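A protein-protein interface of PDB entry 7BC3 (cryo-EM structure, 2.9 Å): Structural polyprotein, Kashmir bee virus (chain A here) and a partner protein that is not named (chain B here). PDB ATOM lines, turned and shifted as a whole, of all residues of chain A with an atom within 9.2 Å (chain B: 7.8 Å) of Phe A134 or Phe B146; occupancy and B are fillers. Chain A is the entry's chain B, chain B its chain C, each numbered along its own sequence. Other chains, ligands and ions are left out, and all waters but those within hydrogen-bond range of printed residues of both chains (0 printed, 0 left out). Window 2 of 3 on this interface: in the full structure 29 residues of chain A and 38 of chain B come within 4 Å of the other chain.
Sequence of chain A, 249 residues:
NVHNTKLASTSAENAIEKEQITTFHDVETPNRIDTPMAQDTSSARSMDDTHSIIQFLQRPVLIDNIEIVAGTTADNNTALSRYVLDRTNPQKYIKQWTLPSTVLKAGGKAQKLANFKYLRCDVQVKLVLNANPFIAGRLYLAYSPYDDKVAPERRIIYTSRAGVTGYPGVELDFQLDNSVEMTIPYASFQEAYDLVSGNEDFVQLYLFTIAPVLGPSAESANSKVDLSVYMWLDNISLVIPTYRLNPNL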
ATOM      1  N   ALA A  70     -12.386  -9.996  19.968  1.00  0.00           N
ATOM      2  CA  ALA A  70     -11.989 -11.186  20.702  1.00  0.00           C
ATOM      3  C   ALA A  70     -13.156 -12.155  20.843  1.00  0.00           C
ATOM      4  O   ALA A  70     -14.325 -11.761  20.859  1.00  0.00           O
ATOM      5  CB  ALA A  70     -11.464 -10.805  22.085  1.00  0.00           C
ATOM      6  N   ALA A 131      -4.982  -0.761  19.727  1.00  0.00           N
ATOM      7  CA  ALA A 131      -5.555  -1.655  20.721  1.00  0.00           C
ATOM      8  C   ALA A 131      -5.283  -1.069  22.094  1.00  0.00           C
ATOM      9  O   ALA A 131      -4.162  -0.631  22.369  1.00  0.00           O
ATOM     10  CB  ALA A 131      -4.961  -3.061  20.618  1.00  0.00           C
ATOM     11  N   ASN A 132      -6.303  -1.052  22.943  1.00  0.00           N
ATOM     12  CA  ASN A 132      -6.127  -0.564  24.302  1.00  0.00           C
ATOM     13  C   ASN A 132      -4.999  -1.346  24.963  1.00  0.00           C
ATOM     14  O   ASN A 132      -4.750  -2.501  24.593  1.00  0.00           O
ATOM     15  CB  ASN A 132      -7.423  -0.694  25.103  1.00  0.00           C
ATOM     16  CG  ASN A 132      -8.041  -2.064  24.987  1.00  0.00           C
ATOM     17  OD1 ASN A 132      -7.766  -2.802  24.043  1.00  0.00           O
ATOM     18  ND2 ASN A 132      -8.880  -2.417  25.951  1.00  0.00           N
ATOM     19  N   PRO A 133      -4.295  -0.765  25.934  1.00  0.00           N
ATOM     20  CA  PRO A 133      -3.136  -1.457  26.513  1.00  0.00           C
ATOM     21  C   PRO A 133      -3.487  -2.744  27.244  1.00  0.00           C
ATOM     22  O   PRO A 133      -2.591  -3.479  27.669  1.00  0.00           O
ATOM     23  CB  PRO A 133      -2.557  -0.415  27.478  1.00  0.00           C
ATOM     24  CG  PRO A 133      -3.072   0.881  26.995  1.00  0.00           C
ATOM     25  CD  PRO A 133      -4.429   0.600  26.463  1.00  0.00           C
ATOM     26  N   PHE A 134      -4.777  -3.028  27.399  1.00  0.00           N
ATOM     27  CA  PHE A 134      -5.235  -4.234  28.071  1.00  0.00           C
ATOM     28  C   PHE A 134      -5.535  -5.366  27.099  1.00  0.00           C
ATOM     29  O   PHE A 134      -6.050  -6.407  27.517  1.00  0.00           O
ATOM     30  CB  PHE A 134      -6.475  -3.922  28.908  1.00  0.00           C
ATOM     31  CG  PHE A 134      -6.229  -2.915  29.986  1.00  0.00           C
ATOM     32  CD1 PHE A 134      -5.861  -3.317  31.255  1.00  0.00           C
ATOM     33  CD2 PHE A 134      -6.357  -1.564  29.730  1.00  0.00           C
ATOM     34  CE1 PHE A 134      -5.630  -2.393  32.247  1.00  0.00           C
ATOM     35  CE2 PHE A 134      -6.128  -0.635  30.718  1.00  0.00           C
ATOM     36  CZ  PHE A 134      -5.764  -1.050  31.979  1.00  0.00           C
ATOM     37  N   ILE A 135      -5.223  -5.188  25.820  1.00  0.00           N
ATOM     38  CA  ILE A 135      -5.437  -6.204  24.799  1.00  0.00           C
ATOM     39  C   ILE A 135      -4.094  -6.557  24.182  1.00  0.00           C
ATOM     40  O   ILE A 135      -3.261  -5.679  23.938  1.00  0.00           O
ATOM     41  CB  ILE A 135      -6.428  -5.726  23.719  1.00  0.00           C
ATOM     42  CG1 ILE A 135      -7.833  -5.613  24.305  1.00  0.00           C
ATOM     43  CG2 ILE A 135      -6.422  -6.675  22.539  1.00  0.00           C
ATOM     44  CD1 ILE A 135      -8.519  -6.938  24.517  1.00  0.00           C
ATOM     45  N   ALA A 136      -3.890  -7.847  23.931  1.00  0.00           N
ATOM     46  CA  ALA A 136      -2.644  -8.355  23.389  1.00  0.00           C
ATOM     47  C   ALA A 136      -2.938  -9.252  22.197  1.00  0.00           C
ATOM     48  O   ALA A 136      -4.074  -9.674  21.966  1.00  0.00           O
ATOM     49  CB  ALA A 136      -1.848  -9.128  24.445  1.00  0.00           C
ATOM     50  N   GLY A 137      -1.893  -9.542  21.441  1.00  0.00           N
ATOM     51  CA  GLY A 137      -2.014 -10.380  20.268  1.00  0.00           C
ATOM     52  C   GLY A 137      -0.827 -10.190  19.358  1.00  0.00           C
ATOM     53  O   GLY A 137       0.034  -9.341  19.582  1.00  0.00           O
ATOM     54  N   PHE A 174       0.739  -6.053  19.226  1.00  0.00           N
ATOM     55  CA  PHE A 174      -0.156  -4.944  19.528  1.00  0.00           C
ATOM     56  C   PHE A 174       0.490  -3.920  20.451  1.00  0.00           C
ATOM     57  O   PHE A 174       0.230  -2.720  20.311  1.00  0.00           O
ATOM     58  CB  PHE A 174      -1.449  -5.466  20.155  1.00  0.00           C
ATOM     59  CG  PHE A 174      -2.256  -6.363  19.254  1.00  0.00           C
ATOM     60  CD1 PHE A 174      -1.846  -6.643  17.961  1.00  0.00           C
ATOM     61  CD2 PHE A 174      -3.433  -6.928  19.708  1.00  0.00           C
ATOM     62  CE1 PHE A 174      -2.591  -7.467  17.147  1.00  0.00           C
ATOM     63  CE2 PHE A 174      -4.180  -7.752  18.894  1.00  0.00           C
ATOM     64  CZ  PHE A 174      -3.758  -8.020  17.615  1.00  0.00           C
ATOM     65  N   GLN A 175       1.327  -4.364  21.387  1.00  0.00           N
ATOM     66  CA  GLN A 175       1.934  -3.483  22.376  1.00  0.00           C
ATOM     67  C   GLN A 175       3.411  -3.225  22.112  1.00  0.00           C
ATOM     68  O   GLN A 175       4.083  -2.620  22.953  1.00  0.00           O
ATOM     69  CB  GLN A 175       1.749  -4.066  23.777  1.00  0.00           C
ATOM     70  CG  GLN A 175       0.305  -4.356  24.148  1.00  0.00           C
ATOM     71  CD  GLN A 175      -0.618  -3.181  23.895  1.00  0.00           C
ATOM     72  OE1 GLN A 175      -0.196  -2.027  23.926  1.00  0.00           O
ATOM     73  NE2 GLN A 175      -1.886  -3.473  23.642  1.00  0.00           N
ATOM     74  N   VAL A 213      -6.579 -12.534  19.473  1.00  0.00           N
ATOM     75  CA  VAL A 213      -6.711 -11.378  20.350  1.00  0.00           C
ATOM     76  C   VAL A 213      -6.975 -11.866  21.765  1.00  0.00           C
ATOM     77  O   VAL A 213      -7.908 -12.642  22.009  1.00  0.00           O
ATOM     78  CB  VAL A 213      -7.821 -10.447  19.858  1.00  0.00           C
ATOM     79  CG1 VAL A 213      -8.054  -9.327  20.854  1.00  0.00           C
ATOM     80  CG2 VAL A 213      -7.466  -9.882  18.496  1.00  0.00           C
ATOM     81  N   LEU A 214      -6.153 -11.414  22.707  1.00  0.00           N
ATOM     82  CA  LEU A 214      -6.244 -11.818  24.104  1.00  0.00           C
ATOM     83  C   LEU A 214      -6.752 -10.637  24.918  1.00  0.00           C
ATOM     84  O   LEU A 214      -6.063  -9.619  25.046  1.00  0.00           O
ATOM     85  CB  LEU A 214      -4.891 -12.292  24.624  1.00  0.00           C
ATOM     86  CG  LEU A 214      -4.230 -13.429  23.848  1.00  0.00           C
ATOM     87  CD1 LEU A 214      -2.841 -13.690  24.394  1.00  0.00           C
ATOM     88  CD2 LEU A 214      -5.078 -14.690  23.901  1.00  0.00           C
ATOM     89  N   GLY A 215      -7.954 -10.777  25.466  1.00  0.00           N
ATOM     90  CA  GLY A 215      -8.527  -9.766  26.317  1.00  0.00           C
ATOM     91  C   GLY A 215      -9.225 -10.378  27.510  1.00  0.00           C
ATOM     92  O   GLY A 215      -9.339 -11.601  27.634  1.00  0.00           O
ATOM     93  N   PRO A 216      -9.711  -9.533  28.414  1.00  0.00           N
ATOM     94  CA  PRO A 216     -10.406 -10.047  29.597  1.00  0.00           C
ATOM     95  C   PRO A 216     -11.688 -10.773  29.217  1.00  0.00           C
ATOM     96  O   PRO A 216     -12.253 -10.578  28.140  1.00  0.00           O
ATOM     97  CB  PRO A 216     -10.698  -8.784  30.415  1.00  0.00           C
ATOM     98  CG  PRO A 216     -10.680  -7.678  29.425  1.00  0.00           C
ATOM     99  CD  PRO A 216      -9.693  -8.064  28.374  1.00  0.00           C
ATOM    100  N   SER A 217     -12.146 -11.625  30.133  1.00  0.00           N
ATOM    101  CA  SER A 217     -13.375 -12.390  29.933  1.00  0.00           C
ATOM    102  C   SER A 217     -14.593 -11.513  30.232  1.00  0.00           C
ATOM    103  O   SER A 217     -15.418 -11.801  31.097  1.00  0.00           O
ATOM    104  CB  SER A 217     -13.361 -13.640  30.802  1.00  0.00           C
ATOM    105  OG  SER A 217     -12.308 -14.507  30.426  1.00  0.00           O
ATOM    106  N   ASN A 222     -15.221  -3.819  24.170  1.00  0.00           N
ATOM    107  CA  ASN A 222     -13.954  -3.102  24.178  1.00  0.00           C
ATOM    108  C   ASN A 222     -12.755  -3.988  23.873  1.00  0.00           C
ATOM    109  O   ASN A 222     -11.697  -3.463  23.510  1.00  0.00           O
ATOM    110  CB  ASN A 222     -13.738  -2.426  25.538  1.00  0.00           C
ATOM    111  CG  ASN A 222     -14.735  -1.316  25.800  1.00  0.00           C
ATOM    112  OD1 ASN A 222     -15.477  -1.352  26.781  1.00  0.00           O
ATOM    113  ND2 ASN A 222     -14.758  -0.319  24.922  1.00  0.00           N
ATOM    114  N   SER A 223     -12.889  -5.304  24.010  1.00  0.00           N
ATOM    115  CA  SER A 223     -11.795  -6.232  23.732  1.00  0.00           C
ATOM    116  C   SER A 223     -11.743  -6.464  22.229  1.00  0.00           C
ATOM    117  O   SER A 223     -12.399  -7.355  21.689  1.00  0.00           O
ATOM    118  CB  SER A 223     -11.989  -7.535  24.495  1.00  0.00           C
ATOM    119  OG  SER A 223     -11.965  -7.314  25.894  1.00  0.00           O
ATOM    120  N   LYS A 224     -10.946  -5.651  21.544  1.00  0.00           N
ATOM    121  CA  LYS A 224     -10.892  -5.677  20.088  1.00  0.00           C
ATOM    122  C   LYS A 224      -9.655  -4.917  19.634  1.00  0.00           C
ATOM    123  O   LYS A 224      -9.001  -4.224  20.418  1.00  0.00           O
ATOM    124  CB  LYS A 224     -12.152  -5.065  19.479  1.00  0.00           C
ATOM    125  CG  LYS A 224     -12.190  -3.559  19.587  1.00  0.00           C
ATOM    126  CD  LYS A 224     -13.602  -3.032  19.483  1.00  0.00           C
ATOM    127  CE  LYS A 224     -13.620  -1.594  19.006  1.00  0.00           C
ATOM    128  NZ  LYS A 224     -14.854  -0.890  19.438  1.00  0.00           N
ATOM    129  N   LYS B 143       2.026 -10.443  25.578  1.00  0.00           N
ATOM    130  CA  LYS B 143       1.415 -10.017  26.824  1.00  0.00           C
ATOM    131  C   LYS B 143       1.127  -8.524  26.743  1.00  0.00           C
ATOM    132  O   LYS B 143       1.158  -7.923  25.665  1.00  0.00           O
ATOM    133  CB  LYS B 143       2.333 -10.352  28.004  1.00  0.00           C
ATOM    134  CG  LYS B 143       3.657  -9.624  27.946  1.00  0.00           C
ATOM    135  CD  LYS B 143       4.466  -9.817  29.199  1.00  0.00           C
ATOM    136  CE  LYS B 143       5.488  -8.714  29.332  1.00  0.00           C
ATOM    137  NZ  LYS B 143       4.970  -7.548  30.090  1.00  0.00           N
ATOM    138  N   THR B 144       0.847  -7.929  27.895  1.00  0.00           N
ATOM    139  CA  THR B 144       0.673  -6.494  28.050  1.00  0.00           C
ATOM    140  C   THR B 144       1.688  -5.977  29.062  1.00  0.00           C
ATOM    141  O   THR B 144       2.564  -6.708  29.530  1.00  0.00           O
ATOM    142  CB  THR B 144      -0.750  -6.152  28.500  1.00  0.00           C
ATOM    143  OG1 THR B 144      -0.931  -6.549  29.864  1.00  0.00           O
ATOM    144  CG2 THR B 144      -1.777  -6.850  27.639  1.00  0.00           C
ATOM    145  N   ALA B 145       1.560  -4.699  29.402  1.00  0.00           N
ATOM    146  CA  ALA B 145       2.379  -4.100  30.445  1.00  0.00           C
ATOM    147  C   ALA B 145       1.881  -4.431  31.843  1.00  0.00           C
ATOM    148  O   ALA B 145       2.493  -3.991  32.821  1.00  0.00           O
ATOM    149  CB  ALA B 145       2.428  -2.584  30.263  1.00  0.00           C
ATOM    150  N   PHE B 146       0.796  -5.193  31.960  1.00  0.00           N
ATOM    151  CA  PHE B 146       0.204  -5.534  33.243  1.00  0.00           C
ATOM    152  C   PHE B 146       0.323  -7.013  33.573  1.00  0.00           C
ATOM    153  O   PHE B 146      -0.107  -7.430  34.652  1.00  0.00           O
ATOM    154  CB  PHE B 146      -1.264  -5.103  33.259  1.00  0.00           C
ATOM    155  CG  PHE B 146      -1.486  -3.735  32.692  1.00  0.00           C
ATOM    156  CD1 PHE B 146      -1.382  -2.614  33.493  1.00  0.00           C
ATOM    157  CD2 PHE B 146      -1.777  -3.568  31.351  1.00  0.00           C
ATOM    158  CE1 PHE B 146      -1.575  -1.355  32.971  1.00  0.00           C
ATOM    159  CE2 PHE B 146      -1.971  -2.310  30.824  1.00  0.00           C
ATOM    160  CZ  PHE B 146      -1.870  -1.203  31.635  1.00  0.00           C
ATOM    161  N   HIS B 147       0.885  -7.813  32.673  1.00  0.00           N
ATOM    162  CA  HIS B 147       1.290  -9.173  32.989  1.00  0.00           C
ATOM    163  C   HIS B 147       2.712  -9.149  33.528  1.00  0.00           C
ATOM    164  O   HIS B 147       3.585  -8.485  32.960  1.00  0.00           O
ATOM    165  CB  HIS B 147       1.227 -10.069  31.753  1.00  0.00           C
ATOM    166  CG  HIS B 147      -0.152 -10.271  31.210  1.00  0.00           C
ATOM    167  ND1 HIS B 147      -0.646  -9.548  30.147  1.00  0.00           N
ATOM    168  CD2 HIS B 147      -1.132 -11.133  31.567  1.00  0.00           C
ATOM    169  CE1 HIS B 147      -1.876  -9.946  29.880  1.00  0.00           C
ATOM    170  NE2 HIS B 147      -2.195 -10.907  30.728  1.00  0.00           N
ATOM    171  N   THR B 148       2.943  -9.870  34.621  1.00  0.00           N
ATOM    172  CA  THR B 148       4.283 -10.030  35.160  1.00  0.00           C
ATOM    173  C   THR B 148       4.502 -11.494  35.504  1.00  0.00           C
ATOM    174  O   THR B 148       3.557 -12.248  35.745  1.00  0.00           O
ATOM    175  CB  THR B 148       4.525  -9.158  36.401  1.00  0.00           C
ATOM    176  OG1 THR B 148       3.730  -9.632  37.492  1.00  0.00           O
ATOM    177  CG2 THR B 148       4.175  -7.712  36.121  1.00  0.00           C
ATOM    178  N   GLY B 149       5.766 -11.886  35.515  1.00  0.00           N
ATOM    179  CA  GLY B 149       6.125 -13.255  35.812  1.00  0.00           C
ATOM    180  C   GLY B 149       7.597 -13.468  35.570  1.00  0.00           C
ATOM    181  O   GLY B 149       8.288 -12.631  34.983  1.00  0.00           O
ATOM    182  N   LEU B 193       9.215 -10.696  33.140  1.00  0.00           N
ATOM    183  CA  LEU B 193       8.222 -10.229  32.184  1.00  0.00           C
ATOM    184  C   LEU B 193       7.607  -8.896  32.574  1.00  0.00           C
ATOM    185  O   LEU B 193       6.642  -8.462  31.938  1.00  0.00           O
ATOM    186  CB  LEU B 193       7.116 -11.270  32.036  1.00  0.00           C
ATOM    187  CG  LEU B 193       7.216 -12.223  30.854  1.00  0.00           C
ATOM    188  CD1 LEU B 193       8.583 -12.859  30.793  1.00  0.00           C
ATOM    189  CD2 LEU B 193       6.141 -13.265  30.999  1.00  0.00           C
ATOM    190  N   THR B 194       8.125  -8.244  33.612  1.00  0.00           N
ATOM    191  CA  THR B 194       7.545  -6.981  34.053  1.00  0.00           C
ATOM    192  C   THR B 194       7.408  -6.007  32.892  1.00  0.00           C
ATOM    193  O   THR B 194       6.327  -5.462  32.643  1.00  0.00           O
ATOM    194  CB  THR B 194       8.405  -6.377  35.158  1.00  0.00           C
ATOM    195  OG1 THR B 194       8.698  -7.378  36.141  1.00  0.00           O
ATOM    196  CG2 THR B 194       7.698  -5.214  35.816  1.00  0.00           C
ATOM    197  N   ASN B 195       8.493  -5.779  32.173  1.00  0.00           N
ATOM    198  CA  ASN B 195       8.491  -4.907  31.004  1.00  0.00           C
ATOM    199  C   ASN B 195       9.014  -5.597  29.755  1.00  0.00           C
ATOM    200  O   ASN B 195       8.494  -5.355  28.664  1.00  0.00           O
ATOM    201  CB  ASN B 195       9.328  -3.654  31.285  1.00  0.00           C
ATOM    202  CG  ASN B 195       8.716  -2.772  32.351  1.00  0.00           C
ATOM    203  OD1 ASN B 195       7.782  -3.171  33.045  1.00  0.00           O
ATOM    204  ND2 ASN B 195       9.242  -1.566  32.488  1.00  0.00           N
ATOM    205  N   LEU B 244       1.966 -16.789  36.721  1.00  0.00           N
ATOM    206  CA  LEU B 244       1.631 -15.629  35.910  1.00  0.00           C
ATOM    207  C   LEU B 244       0.753 -14.682  36.712  1.00  0.00           C
ATOM    208  O   LEU B 244      -0.260 -15.089  37.289  1.00  0.00           O
ATOM    209  CB  LEU B 244       0.923 -16.051  34.626  1.00  0.00           C
ATOM    210  CG  LEU B 244       0.539 -14.885  33.712  1.00  0.00           C
ATOM    211  CD1 LEU B 244       1.777 -14.206  33.160  1.00  0.00           C
ATOM    212  CD2 LEU B 244      -0.356 -15.347  32.589  1.00  0.00           C
ATOM    213  N   MET B 245       1.147 -13.417  36.745  1.00  0.00           N
ATOM    214  CA  MET B 245       0.435 -12.387  37.484  1.00  0.00           C
ATOM    215  C   MET B 245      -0.357 -11.545  36.497  1.00  0.00           C
ATOM    216  O   MET B 245       0.216 -10.972  35.565  1.00  0.00           O
ATOM    217  CB  MET B 245       1.410 -11.517  38.271  1.00  0.00           C
ATOM    218  CG  MET B 245       2.182 -12.267  39.334  1.00  0.00           C
ATOM    219  SD  MET B 245       1.287 -12.370  40.889  1.00  0.00           S
ATOM    220  CE  MET B 245       1.369 -14.132  41.169  1.00  0.00           C
ATOM    221  N   ALA B 246      -1.662 -11.472  36.702  1.00  0.00           N
ATOM    222  CA  ALA B 246      -2.521 -10.745  35.786  1.00  0.00           C
ATOM    223  C   ALA B 246      -3.802 -10.327  36.493  1.00  0.00           C
ATOM    224  O   ALA B 246      -4.504 -11.178  37.053  1.00  0.00           O
ATOM    225  CB  ALA B 246      -2.845 -11.604  34.565  1.00  0.00           C
ATOM    226  N   PRO B 247      -4.145  -9.039  36.498  1.00  0.00           N
ATOM    227  CA  PRO B 247      -5.447  -8.644  37.043  1.00  0.00           C
ATOM    228  C   PRO B 247      -6.582  -9.121  36.157  1.00  0.00           C
ATOM    229  O   PRO B 247      -6.344  -9.653  35.069  1.00  0.00           O
ATOM    230  CB  PRO B 247      -5.363  -7.114  37.091  1.00  0.00           C
ATOM    231  CG  PRO B 247      -4.322  -6.755  36.106  1.00  0.00           C
ATOM    232  CD  PRO B 247      -3.341  -7.873  36.097  1.00  0.00           C
ATOM    233  N   ASP B 248      -7.819  -8.937  36.606  1.00  0.00           N
ATOM    234  CA  ASP B 248      -8.976  -9.360  35.830  1.00  0.00           C
ATOM    235  C   ASP B 248      -9.348  -8.367  34.739  1.00  0.00           C
ATOM    236  O   ASP B 248     -10.379  -8.548  34.084  1.00  0.00           O
ATOM    237  CB  ASP B 248     -10.165  -9.591  36.763  1.00  0.00           C
ATOM    238  CG  ASP B 248      -9.776 -10.323  38.030  1.00  0.00           C
ATOM    239  OD1 ASP B 248      -9.316 -11.479  37.931  1.00  0.00           O
ATOM    240  OD2 ASP B 248      -9.927  -9.741  39.125  1.00  0.00           O
ATOM    241  N   THR B 249      -8.537  -7.332  34.531  1.00  0.00           N
ATOM    242  CA  THR B 249      -8.725  -6.397  33.434  1.00  0.00           C
ATOM    243  C   THR B 249      -8.019  -6.838  32.160  1.00  0.00           C
ATOM    244  O   THR B 249      -8.272  -6.262  31.097  1.00  0.00           O
ATOM    245  CB  THR B 249      -8.215  -5.007  33.827  1.00  0.00           C
ATOM    246  OG1 THR B 249      -6.801  -5.061  34.051  1.00  0.00           O
ATOM    247  CG2 THR B 249      -8.903  -4.513  35.086  1.00  0.00           C
ATOM    248  N   VAL B 250      -7.143  -7.838  32.244  1.00  0.00           N
ATOM    249  CA  VAL B 250      -6.423  -8.351  31.087  1.00  0.00           C
ATOM    250  C   VAL B 250      -6.715  -9.837  30.949  1.00  0.00           C
ATOM    251  O   VAL B 250      -7.471 -10.409  31.741  1.00  0.00           O
ATOM    252  CB  VAL B 250      -4.909  -8.099  31.208  1.00  0.00           C
ATOM    253  CG1 VAL B 250      -4.606  -6.622  31.118  1.00  0.00           C
ATOM    254  CG2 VAL B 250      -4.371  -8.673  32.507  1.00  0.00           C
ATOM    255  N   SER B 251      -6.121 -10.468  29.943  1.00  0.00           N
ATOM    256  CA  SER B 251      -6.267 -11.903  29.779  1.00  0.00           C
ATOM    257  C   SER B 251      -5.581 -12.639  30.921  1.00  0.00           C
ATOM    258  O   SER B 251      -4.556 -12.200  31.448  1.00  0.00           O
ATOM    259  CB  SER B 251      -5.674 -12.350  28.443  1.00  0.00           C
ATOM    260  OG  SER B 251      -6.072 -13.670  28.122  1.00  0.00           O
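Of the printed residues of chain B, Pro A133 touches Thr B144 (3.4 Å) and Phe B146 (3.4 Å). Printed residues of chain B within 4 Å of Phe A134: Phe B146 (3.9 Å), Thr B249 (3.4 Å) and Val B250 (3.5 Å). Lys A224 touches none of the printed residues of chain B. Of chain A, only Pro A133 and Ala A136 come within 4 Å of Thr B144. No residue of chain A comes within 4 Å of Ala B145. Phe B146 touches two residues of chain A. Printed residues of chain A within 4 Å of Ser B251: Leu A214 and Gly A215. The nearest residue of chain A that does not touch Phe B146 is Ile A135 (6.6 Å). The nearest printed residue of chain A that does not touch Thr B249 is Gly A215 (5.5 Å).
Pro A133 touches Thr B144 (O to CB, 3.4 Å). Phe B146 touches Pro A133. Phe B146 touches Phe A134 (CZ to CZ, 3.9 Å). Phe A134 touches Thr B249 (CD1 to OG1, 3.4 Å). CD1 of Phe A134 touches CG1 of Val B250, at 3.5 Å. Ala A136 touches Lys B143. Thr B144 touches Ala A136 (CG2 to CB, 3.9 Å). Leu A214 touches Ser B251. Gly A215 touches Ser B251. Pro A216 touches Asp B248.
The backbone carbonyl oxygen (O) of Ser B251 lies within hydrogen-bond range of a ring nitrogen (NE2) of His B147. The side-chain amino group (NZ) of Lys B143 sits at hydrogen-bond distance from the backbone carbonyl oxygen (O) of Leu B193 (2.7 Å). OG1 of Thr B144 is in hydrogen-bond range of ND1 of His B147 (3.0 Å). O of Ile A135 lies within hydrogen-bond range of NE2 of Gln A175 (2.6 Å). O of Ala A136 is in hydrogen-bond range of N of Leu A214 (2.8 Å). NZ of Lys B143 is in hydrogen-bond range of O of His B147.
Hydrophobic or aromatic side chains of chain B within 4 Å of the printed part of chain A: Phe B146 and Val B250. Of the 18 printed residues of chain A, 7 touch a printed residue of chain B. Hydrophobic or aromatic side chains of chain A that line the printed part of chain B: Pro A133, Phe A134, Ala A136, Leu A214 and Pro A216. Among the printed residues, 13 pairs touch across the chains. Among the printed residues, no Asp or Glu carboxylate lies within 4 Å of a Lys or Arg side-chain nitrogen of the other chain.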
